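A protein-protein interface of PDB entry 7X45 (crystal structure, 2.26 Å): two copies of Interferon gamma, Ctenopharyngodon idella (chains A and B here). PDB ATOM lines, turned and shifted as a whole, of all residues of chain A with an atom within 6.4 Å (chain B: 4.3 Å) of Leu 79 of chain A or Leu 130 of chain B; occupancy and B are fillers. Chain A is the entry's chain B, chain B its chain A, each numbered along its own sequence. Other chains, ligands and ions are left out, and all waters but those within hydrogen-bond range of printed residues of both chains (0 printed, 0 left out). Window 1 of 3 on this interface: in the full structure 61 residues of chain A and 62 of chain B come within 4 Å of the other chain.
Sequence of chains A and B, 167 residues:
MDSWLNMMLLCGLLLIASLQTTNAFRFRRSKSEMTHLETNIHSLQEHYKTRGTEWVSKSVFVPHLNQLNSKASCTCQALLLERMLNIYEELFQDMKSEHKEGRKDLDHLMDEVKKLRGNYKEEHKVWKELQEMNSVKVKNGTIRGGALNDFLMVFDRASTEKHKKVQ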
ATOM      1  N   CYS A  74       4.992  15.340  18.275  1.00  0.00           N
ATOM      2  CA  CYS A  74       5.346  16.751  17.955  1.00  0.00           C
ATOM      3  C   CYS A  74       4.097  17.586  17.662  1.00  0.00           C
ATOM      4  O   CYS A  74       3.386  17.255  16.717  1.00  0.00           O
ATOM      5  CB  CYS A  74       6.290  16.761  16.759  1.00  0.00           C
ATOM      6  SG  CYS A  74       6.918  18.396  16.317  1.00  0.00           S
ATOM      7  N   THR A  75       3.871  18.658  18.424  1.00  0.00           N
ATOM      8  CA  THR A  75       2.747  19.620  18.215  1.00  0.00           C
ATOM      9  C   THR A  75       3.280  20.913  17.598  1.00  0.00           C
ATOM     10  O   THR A  75       4.477  21.189  17.721  1.00  0.00           O
ATOM     11  CB  THR A  75       1.978  19.867  19.518  1.00  0.00           C
ATOM     12  OG1 THR A  75       2.641  20.861  20.284  1.00  0.00           O
ATOM     13  CG2 THR A  75       1.858  18.621  20.365  1.00  0.00           C
ATOM     14  N   CYS A  76       2.411  21.687  16.952  1.00  0.00           N
ATOM     15  CA  CYS A  76       2.773  22.997  16.353  1.00  0.00           C
ATOM     16  C   CYS A  76       3.041  24.021  17.458  1.00  0.00           C
ATOM     17  O   CYS A  76       3.922  24.871  17.264  1.00  0.00           O
ATOM     18  CB  CYS A  76       1.687  23.500  15.417  1.00  0.00           C
ATOM     19  SG  CYS A  76       1.529  22.518  13.902  1.00  0.00           S
ATOM     20  N   GLN A  77       2.296  23.970  18.567  1.00  0.00           N
ATOM     21  CA  GLN A  77       2.541  24.863  19.733  1.00  0.00           C
ATOM     22  C   GLN A  77       4.018  24.726  20.109  1.00  0.00           C
ATOM     23  O   GLN A  77       4.732  25.763  20.159  1.00  0.00           O
ATOM     24  CB  GLN A  77       1.619  24.513  20.908  1.00  0.00           C
ATOM     25  CG  GLN A  77       0.184  24.991  20.720  1.00  0.00           C
ATOM     26  CD  GLN A  77      -0.734  24.598  21.855  1.00  0.00           C
ATOM     27  OE1 GLN A  77      -0.519  23.601  22.538  1.00  0.00           O
ATOM     28  NE2 GLN A  77      -1.782  25.383  22.067  1.00  0.00           N
ATOM     29  N   ALA A  78       4.480  23.485  20.294  1.00  0.00           N
ATOM     30  CA  ALA A  78       5.860  23.178  20.740  1.00  0.00           C
ATOM     31  C   ALA A  78       6.865  23.638  19.682  1.00  0.00           C
ATOM     32  O   ALA A  78       7.960  24.097  20.058  1.00  0.00           O
ATOM     33  CB  ALA A  78       6.020  21.706  21.054  1.00  0.00           C
ATOM     34  N   LEU A  79       6.536  23.524  18.403  1.00  0.00           N
ATOM     35  CA  LEU A  79       7.472  23.917  17.323  1.00  0.00           C
ATOM     36  C   LEU A  79       7.603  25.457  17.303  1.00  0.00           C
ATOM     37  O   LEU A  79       8.706  25.963  17.119  1.00  0.00           O
ATOM     38  CB  LEU A  79       6.925  23.325  16.024  1.00  0.00           C
ATOM     39  CG  LEU A  79       7.788  23.500  14.783  1.00  0.00           C
ATOM     40  CD1 LEU A  79       9.045  22.660  14.875  1.00  0.00           C
ATOM     41  CD2 LEU A  79       7.000  23.141  13.532  1.00  0.00           C
ATOM     42  N   LEU A  80       6.518  26.191  17.543  1.00  0.00           N
ATOM     43  CA  LEU A  80       6.540  27.669  17.693  1.00  0.00           C
ATOM     44  C   LEU A  80       7.374  28.079  18.916  1.00  0.00           C
ATOM     45  O   LEU A  80       8.250  28.952  18.771  1.00  0.00           O
ATOM     46  CB  LEU A  80       5.096  28.181  17.760  1.00  0.00           C
ATOM     47  CG  LEU A  80       4.394  28.164  16.403  1.00  0.00           C
ATOM     48  CD1 LEU A  80       2.885  28.175  16.550  1.00  0.00           C
ATOM     49  CD2 LEU A  80       4.874  29.328  15.538  1.00  0.00           C
ATOM     50  N   LEU A  81       7.169  27.437  20.061  1.00  0.00           N
ATOM     51  CA  LEU A  81       7.972  27.693  21.288  1.00  0.00           C
ATOM     52  C   LEU A  81       9.453  27.390  21.012  1.00  0.00           C
ATOM     53  O   LEU A  81      10.319  28.203  21.442  1.00  0.00           O
ATOM     54  CB  LEU A  81       7.418  26.877  22.458  1.00  0.00           C
ATOM     55  CG  LEU A  81       6.030  27.294  22.934  1.00  0.00           C
ATOM     56  CD1 LEU A  81       5.421  26.234  23.839  1.00  0.00           C
ATOM     57  CD2 LEU A  81       6.066  28.646  23.630  1.00  0.00           C
ATOM     58  N   GLU A  82       9.753  26.319  20.273  1.00  0.00           N
ATOM     59  CA  GLU A  82      11.153  25.923  19.954  1.00  0.00           C
ATOM     60  C   GLU A  82      11.806  27.006  19.084  1.00  0.00           C
ATOM     61  O   GLU A  82      12.994  27.264  19.261  1.00  0.00           O
ATOM     62  CB  GLU A  82      11.210  24.562  19.251  1.00  0.00           C
ATOM     63  CG  GLU A  82      12.629  23.996  19.079  1.00  0.00           C
ATOM     64  CD  GLU A  82      13.438  24.443  17.854  1.00  0.00           C
ATOM     65  OE1 GLU A  82      12.844  24.649  16.781  1.00  0.00           O
ATOM     66  OE2 GLU A  82      14.675  24.589  17.967  1.00  0.00           O
ATOM     67  N   ARG A  83      11.073  27.615  18.151  1.00  0.00           N
ATOM     68  CA  ARG A  83      11.641  28.677  17.286  1.00  0.00           C
ATOM     69  C   ARG A  83      12.051  29.833  18.189  1.00  0.00           C
ATOM     70  O   ARG A  83      13.127  30.397  17.971  1.00  0.00           O
ATOM     71  CB  ARG A  83      10.673  29.209  16.231  1.00  0.00           C
ATOM     72  CG  ARG A  83      11.397  29.891  15.082  1.00  0.00           C
ATOM     73  CD  ARG A  83      11.794  28.889  14.004  1.00  0.00           C
ATOM     74  NE  ARG A  83      12.470  27.700  14.517  1.00  0.00           N
ATOM     75  CZ  ARG A  83      13.766  27.637  14.821  1.00  0.00           C
ATOM     76  NH1 ARG A  83      14.526  28.695  14.692  1.00  0.00           N
ATOM     77  NH2 ARG A  83      14.289  26.514  15.280  1.00  0.00           N
ATOM     78  N   MET A  84      11.205  30.174  19.160  1.00  0.00           N
ATOM     79  CA  MET A  84      11.424  31.341  20.047  1.00  0.00           C
ATOM     80  C   MET A  84      12.686  31.102  20.873  1.00  0.00           C
ATOM     81  O   MET A  84      13.519  32.016  20.930  1.00  0.00           O
ATOM     82  CB  MET A  84      10.214  31.572  20.942  1.00  0.00           C
ATOM     83  CG  MET A  84       9.026  32.005  20.133  1.00  0.00           C
ATOM     84  SD  MET A  84       7.654  32.447  21.182  1.00  0.00           S
ATOM     85  CE  MET A  84       6.355  31.399  20.533  1.00  0.00           C
ATOM     86  N   ILE A  87      15.738  31.546  18.781  1.00  0.00           N
ATOM     87  CA  ILE A  87      16.008  32.997  18.519  1.00  0.00           C
ATOM     88  C   ILE A  87      16.647  33.614  19.765  1.00  0.00           C
ATOM     89  O   ILE A  87      17.542  34.471  19.615  1.00  0.00           O
ATOM     90  CB  ILE A  87      14.737  33.743  18.050  1.00  0.00           C
ATOM     91  CG1 ILE A  87      14.287  33.273  16.663  1.00  0.00           C
ATOM     92  CG2 ILE A  87      14.939  35.251  18.071  1.00  0.00           C
ATOM     93  CD1 ILE A  87      12.800  33.395  16.415  1.00  0.00           C
ATOM     94  N   TYR A 120      13.568  19.799  23.294  1.00  0.00           N
ATOM     95  CA  TYR A 120      12.866  20.203  22.048  1.00  0.00           C
ATOM     96  C   TYR A 120      13.660  19.717  20.822  1.00  0.00           C
ATOM     97  O   TYR A 120      13.578  20.359  19.750  1.00  0.00           O
ATOM     98  CB  TYR A 120      12.719  21.728  22.014  1.00  0.00           C
ATOM     99  CG  TYR A 120      11.637  22.302  22.897  1.00  0.00           C
ATOM    100  CD1 TYR A 120      10.396  22.583  22.366  1.00  0.00           C
ATOM    101  CD2 TYR A 120      11.863  22.646  24.225  1.00  0.00           C
ATOM    102  CE1 TYR A 120       9.368  23.099  23.138  1.00  0.00           C
ATOM    103  CE2 TYR A 120      10.857  23.194  25.007  1.00  0.00           C
ATOM    104  CZ  TYR A 120       9.604  23.434  24.454  1.00  0.00           C
ATOM    105  OH  TYR A 120       8.563  23.969  25.148  1.00  0.00           O
ATOM    106  N   GLU A 122      13.256  16.998  18.927  1.00  0.00           N
ATOM    107  CA  GLU A 122      12.388  16.470  17.841  1.00  0.00           C
ATOM    108  C   GLU A 122      11.726  17.649  17.112  1.00  0.00           C
ATOM    109  O   GLU A 122      11.587  17.571  15.876  1.00  0.00           O
ATOM    110  CB  GLU A 122      11.358  15.469  18.377  1.00  0.00           C
ATOM    111  CG  GLU A 122       9.952  16.028  18.569  1.00  0.00           C
ATOM    112  CD  GLU A 122       8.878  15.016  18.959  1.00  0.00           C
ATOM    113  OE1 GLU A 122       8.284  15.182  20.061  1.00  0.00           O
ATOM    114  OE2 GLU A 122       8.606  14.082  18.140  1.00  0.00           O
ATOM    115  N   GLU A 123      11.302  18.675  17.858  1.00  0.00           N
ATOM    116  CA  GLU A 123      10.705  19.925  17.315  1.00  0.00           C
ATOM    117  C   GLU A 123      11.745  20.582  16.401  1.00  0.00           C
ATOM    118  O   GLU A 123      11.406  20.958  15.272  1.00  0.00           O
ATOM    119  CB  GLU A 123      10.253  20.857  18.446  1.00  0.00           C
ATOM    120  CG  GLU A 123       9.011  20.391  19.181  1.00  0.00           C
ATOM    121  CD  GLU A 123       9.209  19.404  20.320  1.00  0.00           C
ATOM    122  OE1 GLU A 123      10.355  18.989  20.577  1.00  0.00           O
ATOM    123  OE2 GLU A 123       8.202  19.046  20.947  1.00  0.00           O
ATOM    124  N   HIS A 124      12.991  20.662  16.845  1.00  0.00           N
ATOM    125  CA  HIS A 124      14.096  21.296  16.079  1.00  0.00           C
ATOM    126  C   HIS A 124      14.295  20.569  14.747  1.00  0.00           C
ATOM    127  O   HIS A 124      14.469  21.279  13.715  1.00  0.00           O
ATOM    128  CB  HIS A 124      15.358  21.396  16.938  1.00  0.00           C
ATOM    129  CG  HIS A 124      16.495  22.058  16.233  1.00  0.00           C
ATOM    130  ND1 HIS A 124      16.555  23.434  16.033  1.00  0.00           N
ATOM    131  CD2 HIS A 124      17.601  21.541  15.648  1.00  0.00           C
ATOM    132  CE1 HIS A 124      17.657  23.731  15.361  1.00  0.00           C
ATOM    133  NE2 HIS A 124      18.317  22.583  15.118  1.00  0.00           N
ATOM    134  N   LYS A 125      14.248  19.227  14.757  1.00  0.00           N
ATOM    135  CA  LYS A 125      14.425  18.338  13.573  1.00  0.00           C
ATOM    136  C   LYS A 125      13.320  18.585  12.554  1.00  0.00           C
ATOM    137  O   LYS A 125      13.590  18.626  11.354  1.00  0.00           O
ATOM    138  CB  LYS A 125      14.319  16.863  13.979  1.00  0.00           C
ATOM    139  CG  LYS A 125      15.559  16.269  14.624  1.00  0.00           C
ATOM    140  CD  LYS A 125      15.580  14.743  14.540  1.00  0.00           C
ATOM    141  CE  LYS A 125      16.979  14.185  14.666  1.00  0.00           C
ATOM    142  NZ  LYS A 125      17.697  14.769  15.826  1.00  0.00           N
ATOM    143  N   VAL A 126      12.092  18.669  13.035  1.00  0.00           N
ATOM    144  CA  VAL A 126      10.913  19.007  12.193  1.00  0.00           C
ATOM    145  C   VAL A 126      11.175  20.340  11.490  1.00  0.00           C
ATOM    146  O   VAL A 126      10.988  20.417  10.259  1.00  0.00           O
ATOM    147  CB  VAL A 126       9.635  19.003  13.042  1.00  0.00           C
ATOM    148  CG1 VAL A 126       8.473  19.700  12.357  1.00  0.00           C
ATOM    149  CG2 VAL A 126       9.269  17.566  13.413  1.00  0.00           C
ATOM    150  N   TRP A 127      11.629  21.347  12.233  1.00  0.00           N
ATOM    151  CA  TRP A 127      11.919  22.682  11.662  1.00  0.00           C
ATOM    152  C   TRP A 127      13.019  22.591  10.598  1.00  0.00           C
ATOM    153  O   TRP A 127      12.874  23.215   9.553  1.00  0.00           O
ATOM    154  CB  TRP A 127      12.302  23.656  12.765  1.00  0.00           C
ATOM    155  CG  TRP A 127      12.914  24.900  12.213  1.00  0.00           C
ATOM    156  CD1 TRP A 127      14.210  25.298  12.319  1.00  0.00           C
ATOM    157  CD2 TRP A 127      12.238  25.914  11.453  1.00  0.00           C
ATOM    158  NE1 TRP A 127      14.379  26.504  11.699  1.00  0.00           N
ATOM    159  CE2 TRP A 127      13.190  26.901  11.152  1.00  0.00           C
ATOM    160  CE3 TRP A 127      10.923  26.088  11.020  1.00  0.00           C
ATOM    161  CZ2 TRP A 127      12.867  28.042  10.421  1.00  0.00           C
ATOM    162  CZ3 TRP A 127      10.604  27.218  10.304  1.00  0.00           C
ATOM    163  CH2 TRP A 127      11.569  28.173   9.999  1.00  0.00           C
ATOM    164  N   LEU A 130      11.423  20.977   7.586  1.00  0.00           N
ATOM    165  CA  LEU A 130      10.623  22.004   6.862  1.00  0.00           C
ATOM    166  C   LEU A 130      11.572  22.902   6.042  1.00  0.00           C
ATOM    167  O   LEU A 130      11.289  23.121   4.848  1.00  0.00           O
ATOM    168  CB  LEU A 130       9.775  22.838   7.828  1.00  0.00           C
ATOM    169  CG  LEU A 130       8.630  22.112   8.558  1.00  0.00           C
ATOM    170  CD1 LEU A 130       8.124  22.932   9.720  1.00  0.00           C
ATOM    171  CD2 LEU A 130       7.461  21.783   7.637  1.00  0.00           C
ATOM    172  N   LEU B  79       1.840  19.745   9.350  1.00  0.00           N
ATOM    173  CA  LEU B  79       2.623  20.922   8.912  1.00  0.00           C
ATOM    174  C   LEU B  79       3.664  20.469   7.868  1.00  0.00           C
ATOM    175  O   LEU B  79       3.843  21.188   6.860  1.00  0.00           O
ATOM    176  CB  LEU B  79       3.248  21.561  10.155  1.00  0.00           C
ATOM    177  CG  LEU B  79       3.948  22.896   9.918  1.00  0.00           C
ATOM    178  CD1 LEU B  79       2.954  23.990   9.552  1.00  0.00           C
ATOM    179  CD2 LEU B  79       4.753  23.300  11.137  1.00  0.00           C
ATOM    180  N   VAL B 126       0.652  28.733  10.594  1.00  0.00           N
ATOM    181  CA  VAL B 126       1.755  28.336  11.509  1.00  0.00           C
ATOM    182  C   VAL B 126       3.096  28.454  10.776  1.00  0.00           C
ATOM    183  O   VAL B 126       4.021  29.069  11.326  1.00  0.00           O
ATOM    184  CB  VAL B 126       1.508  26.921  12.056  1.00  0.00           C
ATOM    185  CG1 VAL B 126       2.747  26.319  12.703  1.00  0.00           C
ATOM    186  CG2 VAL B 126       0.346  26.928  13.036  1.00  0.00           C
ATOM    187  N   TRP B 127       3.189  27.921   9.555  1.00  0.00           N
ATOM    188  CA  TRP B 127       4.443  27.942   8.763  1.00  0.00           C
ATOM    189  C   TRP B 127       4.853  29.392   8.490  1.00  0.00           C
ATOM    190  O   TRP B 127       6.039  29.700   8.641  1.00  0.00           O
ATOM    191  CB  TRP B 127       4.284  27.158   7.465  1.00  0.00           C
ATOM    192  CG  TRP B 127       5.350  27.482   6.467  1.00  0.00           C
ATOM    193  CD1 TRP B 127       5.235  28.228   5.327  1.00  0.00           C
ATOM    194  CD2 TRP B 127       6.732  27.114   6.560  1.00  0.00           C
ATOM    195  NE1 TRP B 127       6.447  28.331   4.706  1.00  0.00           N
ATOM    196  CE2 TRP B 127       7.380  27.652   5.434  1.00  0.00           C
ATOM    197  CE3 TRP B 127       7.478  26.374   7.480  1.00  0.00           C
ATOM    198  CZ2 TRP B 127       8.737  27.447   5.190  1.00  0.00           C
ATOM    199  CZ3 TRP B 127       8.819  26.185   7.246  1.00  0.00           C
ATOM    200  CH2 TRP B 127       9.439  26.716   6.115  1.00  0.00           C
ATOM    201  N   LYS B 128       3.909  30.250   8.102  1.00  0.00           N
ATOM    202  CA  LYS B 128       4.197  31.675   7.793  1.00  0.00           C
ATOM    203  C   LYS B 128       4.630  32.376   9.083  1.00  0.00           C
ATOM    204  O   LYS B 128       5.574  33.195   9.028  1.00  0.00           O
ATOM    205  CB  LYS B 128       2.986  32.347   7.132  1.00  0.00           C
ATOM    206  CG  LYS B 128       2.753  31.972   5.667  1.00  0.00           C
ATOM    207  CD  LYS B 128       4.060  31.903   4.890  1.00  0.00           C
ATOM    208  CE  LYS B 128       3.924  31.738   3.394  1.00  0.00           C
ATOM    209  NZ  LYS B 128       5.254  31.796   2.735  1.00  0.00           N
ATOM    210  N   GLU B 129       4.010  32.017  10.209  1.00  0.00           N
ATOM    211  CA  GLU B 129       4.357  32.553  11.548  1.00  0.00           C
ATOM    212  C   GLU B 129       5.783  32.133  11.873  1.00  0.00           C
ATOM    213  O   GLU B 129       6.596  33.027  12.169  1.00  0.00           O
ATOM    214  CB  GLU B 129       3.371  32.054  12.599  1.00  0.00           C
ATOM    215  CG  GLU B 129       3.325  32.917  13.840  1.00  0.00           C
ATOM    216  CD  GLU B 129       2.239  32.510  14.825  1.00  0.00           C
ATOM    217  OE1 GLU B 129       1.328  31.759  14.418  1.00  0.00           O
ATOM    218  OE2 GLU B 129       2.294  32.940  16.001  1.00  0.00           O
ATOM    219  N   LEU B 130       6.097  30.835  11.782  1.00  0.00           N
ATOM    220  CA  LEU B 130       7.491  30.362  11.997  1.00  0.00           C
ATOM    221  C   LEU B 130       8.458  31.177  11.129  1.00  0.00           C
ATOM    222  O   LEU B 130       9.444  31.678  11.700  1.00  0.00           O
ATOM    223  CB  LEU B 130       7.613  28.871  11.679  1.00  0.00           C
ATOM    224  CG  LEU B 130       6.985  27.906  12.684  1.00  0.00           C
ATOM    225  CD1 LEU B 130       6.852  26.528  12.056  1.00  0.00           C
ATOM    226  CD2 LEU B 130       7.820  27.837  13.965  1.00  0.00           C
ATOM    227  N   GLN B 131       8.217  31.286   9.819  1.00  0.00           N
ATOM    228  CA  GLN B 131       9.114  31.998   8.863  1.00  0.00           C
ATOM    229  C   GLN B 131       9.317  33.446   9.319  1.00  0.00           C
ATOM    230  O   GLN B 131      10.471  33.960   9.240  1.00  0.00           O
ATOM    231  CB  GLN B 131       8.490  32.104   7.469  1.00  0.00           C
ATOM    232  CG  GLN B 131       8.878  31.013   6.481  1.00  0.00           C
ATOM    233  CD  GLN B 131       8.374  31.326   5.081  1.00  0.00           C
ATOM    234  OE1 GLN B 131       7.239  31.775   4.882  1.00  0.00           O
ATOM    235  NE2 GLN B 131       9.206  31.087   4.081  1.00  0.00           N
ATOM    236  N   GLU B 132       8.210  34.095   9.703  1.00  0.00           N
ATOM    237  CA  GLU B 132       8.202  35.520  10.088  1.00  0.00           C
ATOM    238  C   GLU B 132       9.016  35.708  11.364  1.00  0.00           C
ATOM    239  O   GLU B 132       9.835  36.661  11.398  1.00  0.00           O
ATOM    240  CB  GLU B 132       6.795  36.034  10.338  1.00  0.00           C
ATOM    241  CG  GLU B 132       6.825  37.443  10.879  1.00  0.00           C
ATOM    242  CD  GLU B 132       5.494  38.132  10.701  1.00  0.00           C
ATOM    243  OE1 GLU B 132       4.455  37.430  10.793  1.00  0.00           O
ATOM    244  OE2 GLU B 132       5.502  39.345  10.452  1.00  0.00           O
ATOM    245  N   MET B 133       8.765  34.876  12.385  1.00  0.00           N
ATOM    246  CA  MET B 133       9.514  34.950  13.667  1.00  0.00           C
ATOM    247  C   MET B 133      10.993  34.731  13.358  1.00  0.00           C
ATOM    248  O   MET B 133      11.822  35.479  13.888  1.00  0.00           O
ATOM    249  CB  MET B 133       9.098  33.884  14.682  1.00  0.00           C
ATOM    250  CG  MET B 133       7.812  34.195  15.383  1.00  0.00           C
ATOM    251  SD  MET B 133       7.586  33.172  16.840  1.00  0.00           S
ATOM    252  CE  MET B 133       7.365  31.562  16.080  1.00  0.00           C
ATOM    253  N   ASN B 134      11.298  33.702  12.571  1.00  0.00           N
ATOM    254  CA  ASN B 134      12.694  33.245  12.349  1.00  0.00           C
ATOM    255  C   ASN B 134      13.466  34.339  11.610  1.00  0.00           C
ATOM    256  O   ASN B 134      14.671  34.349  11.740  1.00  0.00           O
ATOM    257  CB  ASN B 134      12.749  31.924  11.591  1.00  0.00           C
ATOM    258  CG  ASN B 134      14.043  31.183  11.838  1.00  0.00           C
ATOM    259  OD1 ASN B 134      14.364  30.893  12.989  1.00  0.00           O
ATOM    260  ND2 ASN B 134      14.797  30.903  10.777  1.00  0.00           N
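The side-chain amide oxygen (OD1) of Asn 134 of chain B is in hydrogen-bond range of the guanidinium group (NH1) of Arg 83 of chain A, at 2.8 Å.
The side-chain carboxylate (OE1) of Glu 82 of chain A is in salt-bridge range of the guanidinium group (NH2) of Arg 83 of chain A (2.8 Å).
Of the 20 printed residues of chain A, 7 touch a printed residue of chain B. Printed residues of chain A that touch a printed residue of chain B: Leu 79, Leu 80, Arg 83, Met 84, Ile 87, Trp 127 and Leu 130. Hydrophobic or aromatic side chains of chain A within 4 Å of the printed part of chain B: Leu 79, Leu 80, Met 84, Ile 87, Trp 127 and Leu 130. Hydrophobic or aromatic side chains of chain B that line the printed part of chain A: Leu 79, Trp 127, Leu 130 and Met 133.
CD2 of Leu 79 of chain A touches CD1 of Leu 130 of chain B (3.7 Å). CE of Met 133 of chain B touches CD2 of Leu 80 of chain A (3.4 Å). Leu 130 of chain B touches Arg 83 of chain A (CD2 to CB, 3.9 Å). CG of Met 84 of chain A touches SD of Met 133 of chain B, 3.8 Å away. CD1 of Ile 87 of chain A touches O of Met 133 of chain B (3.4 Å). CZ3 of Trp 127 of chain B touches CZ3 of Trp 127 of chain A (3.7 Å). CZ3 of Trp 127 of chain A touches CB of Leu 130 of chain B, 3.7 Å away. Asn 134 of chain B touches Trp 127 of chain A (ND2 to CZ2, 3.5 Å). Leu 79 of chain B touches Leu 130 of chain A (CD2 to CD1, 3.7 Å). Leu 130 of chain A touches Trp 127 of chain B.
Leu 130 of chain B touches just these residues of chain A: Leu 79, Leu 80, Arg 83 and Trp 127. Of the printed residues of chain A, Trp 127 of chain B touches Trp 127 and Leu 130. Of the printed residues of chain A, Leu 79 of chain B touches Leu 79 (3.3 Å) and Leu 130 (3.7 Å). Of the printed residues of chain B, Met 84 of chain A touches Met 133. Of the printed residues of chain A, Met 133 of chain B touches Leu 80, Met 84 and Ile 87. Of the printed residues of chain A, Asn 134 of chain B touches Arg 83 and Trp 127. Gln 131 of chain B touches none of the printed residues of chain A. Gln 77 of chain A touches none of the printed residues of chain B. The nearest printed residue of chain B that does not touch Leu 79 of chain A is Val 126 of chain B (5.4 Å). The nearest printed residue of chain A that does not touch Trp 127 of chain B is Leu 80 of chain A (6.4 Å).
Leu 79 of chain A touches its own counterpart, Leu 79 of chain B. Leu 79 of chain A touches Leu 130 of chain B, and with the chains exchanged Leu 130 of chain A touches Leu 79 of chain B. Trp 127 of chain A touches its own counterpart, Trp 127 of chain B. Trp 127 of chain A touches Leu 130 of chain B, and with the chains exchanged Leu 130 of chain A touches Trp 127 of chain B. Positions printed for both chains: 79, 126, 127 and 130. Of the 13 pairs that touch across the chains among the printed residues, 6 have their exchanged pair printed and touching as well.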
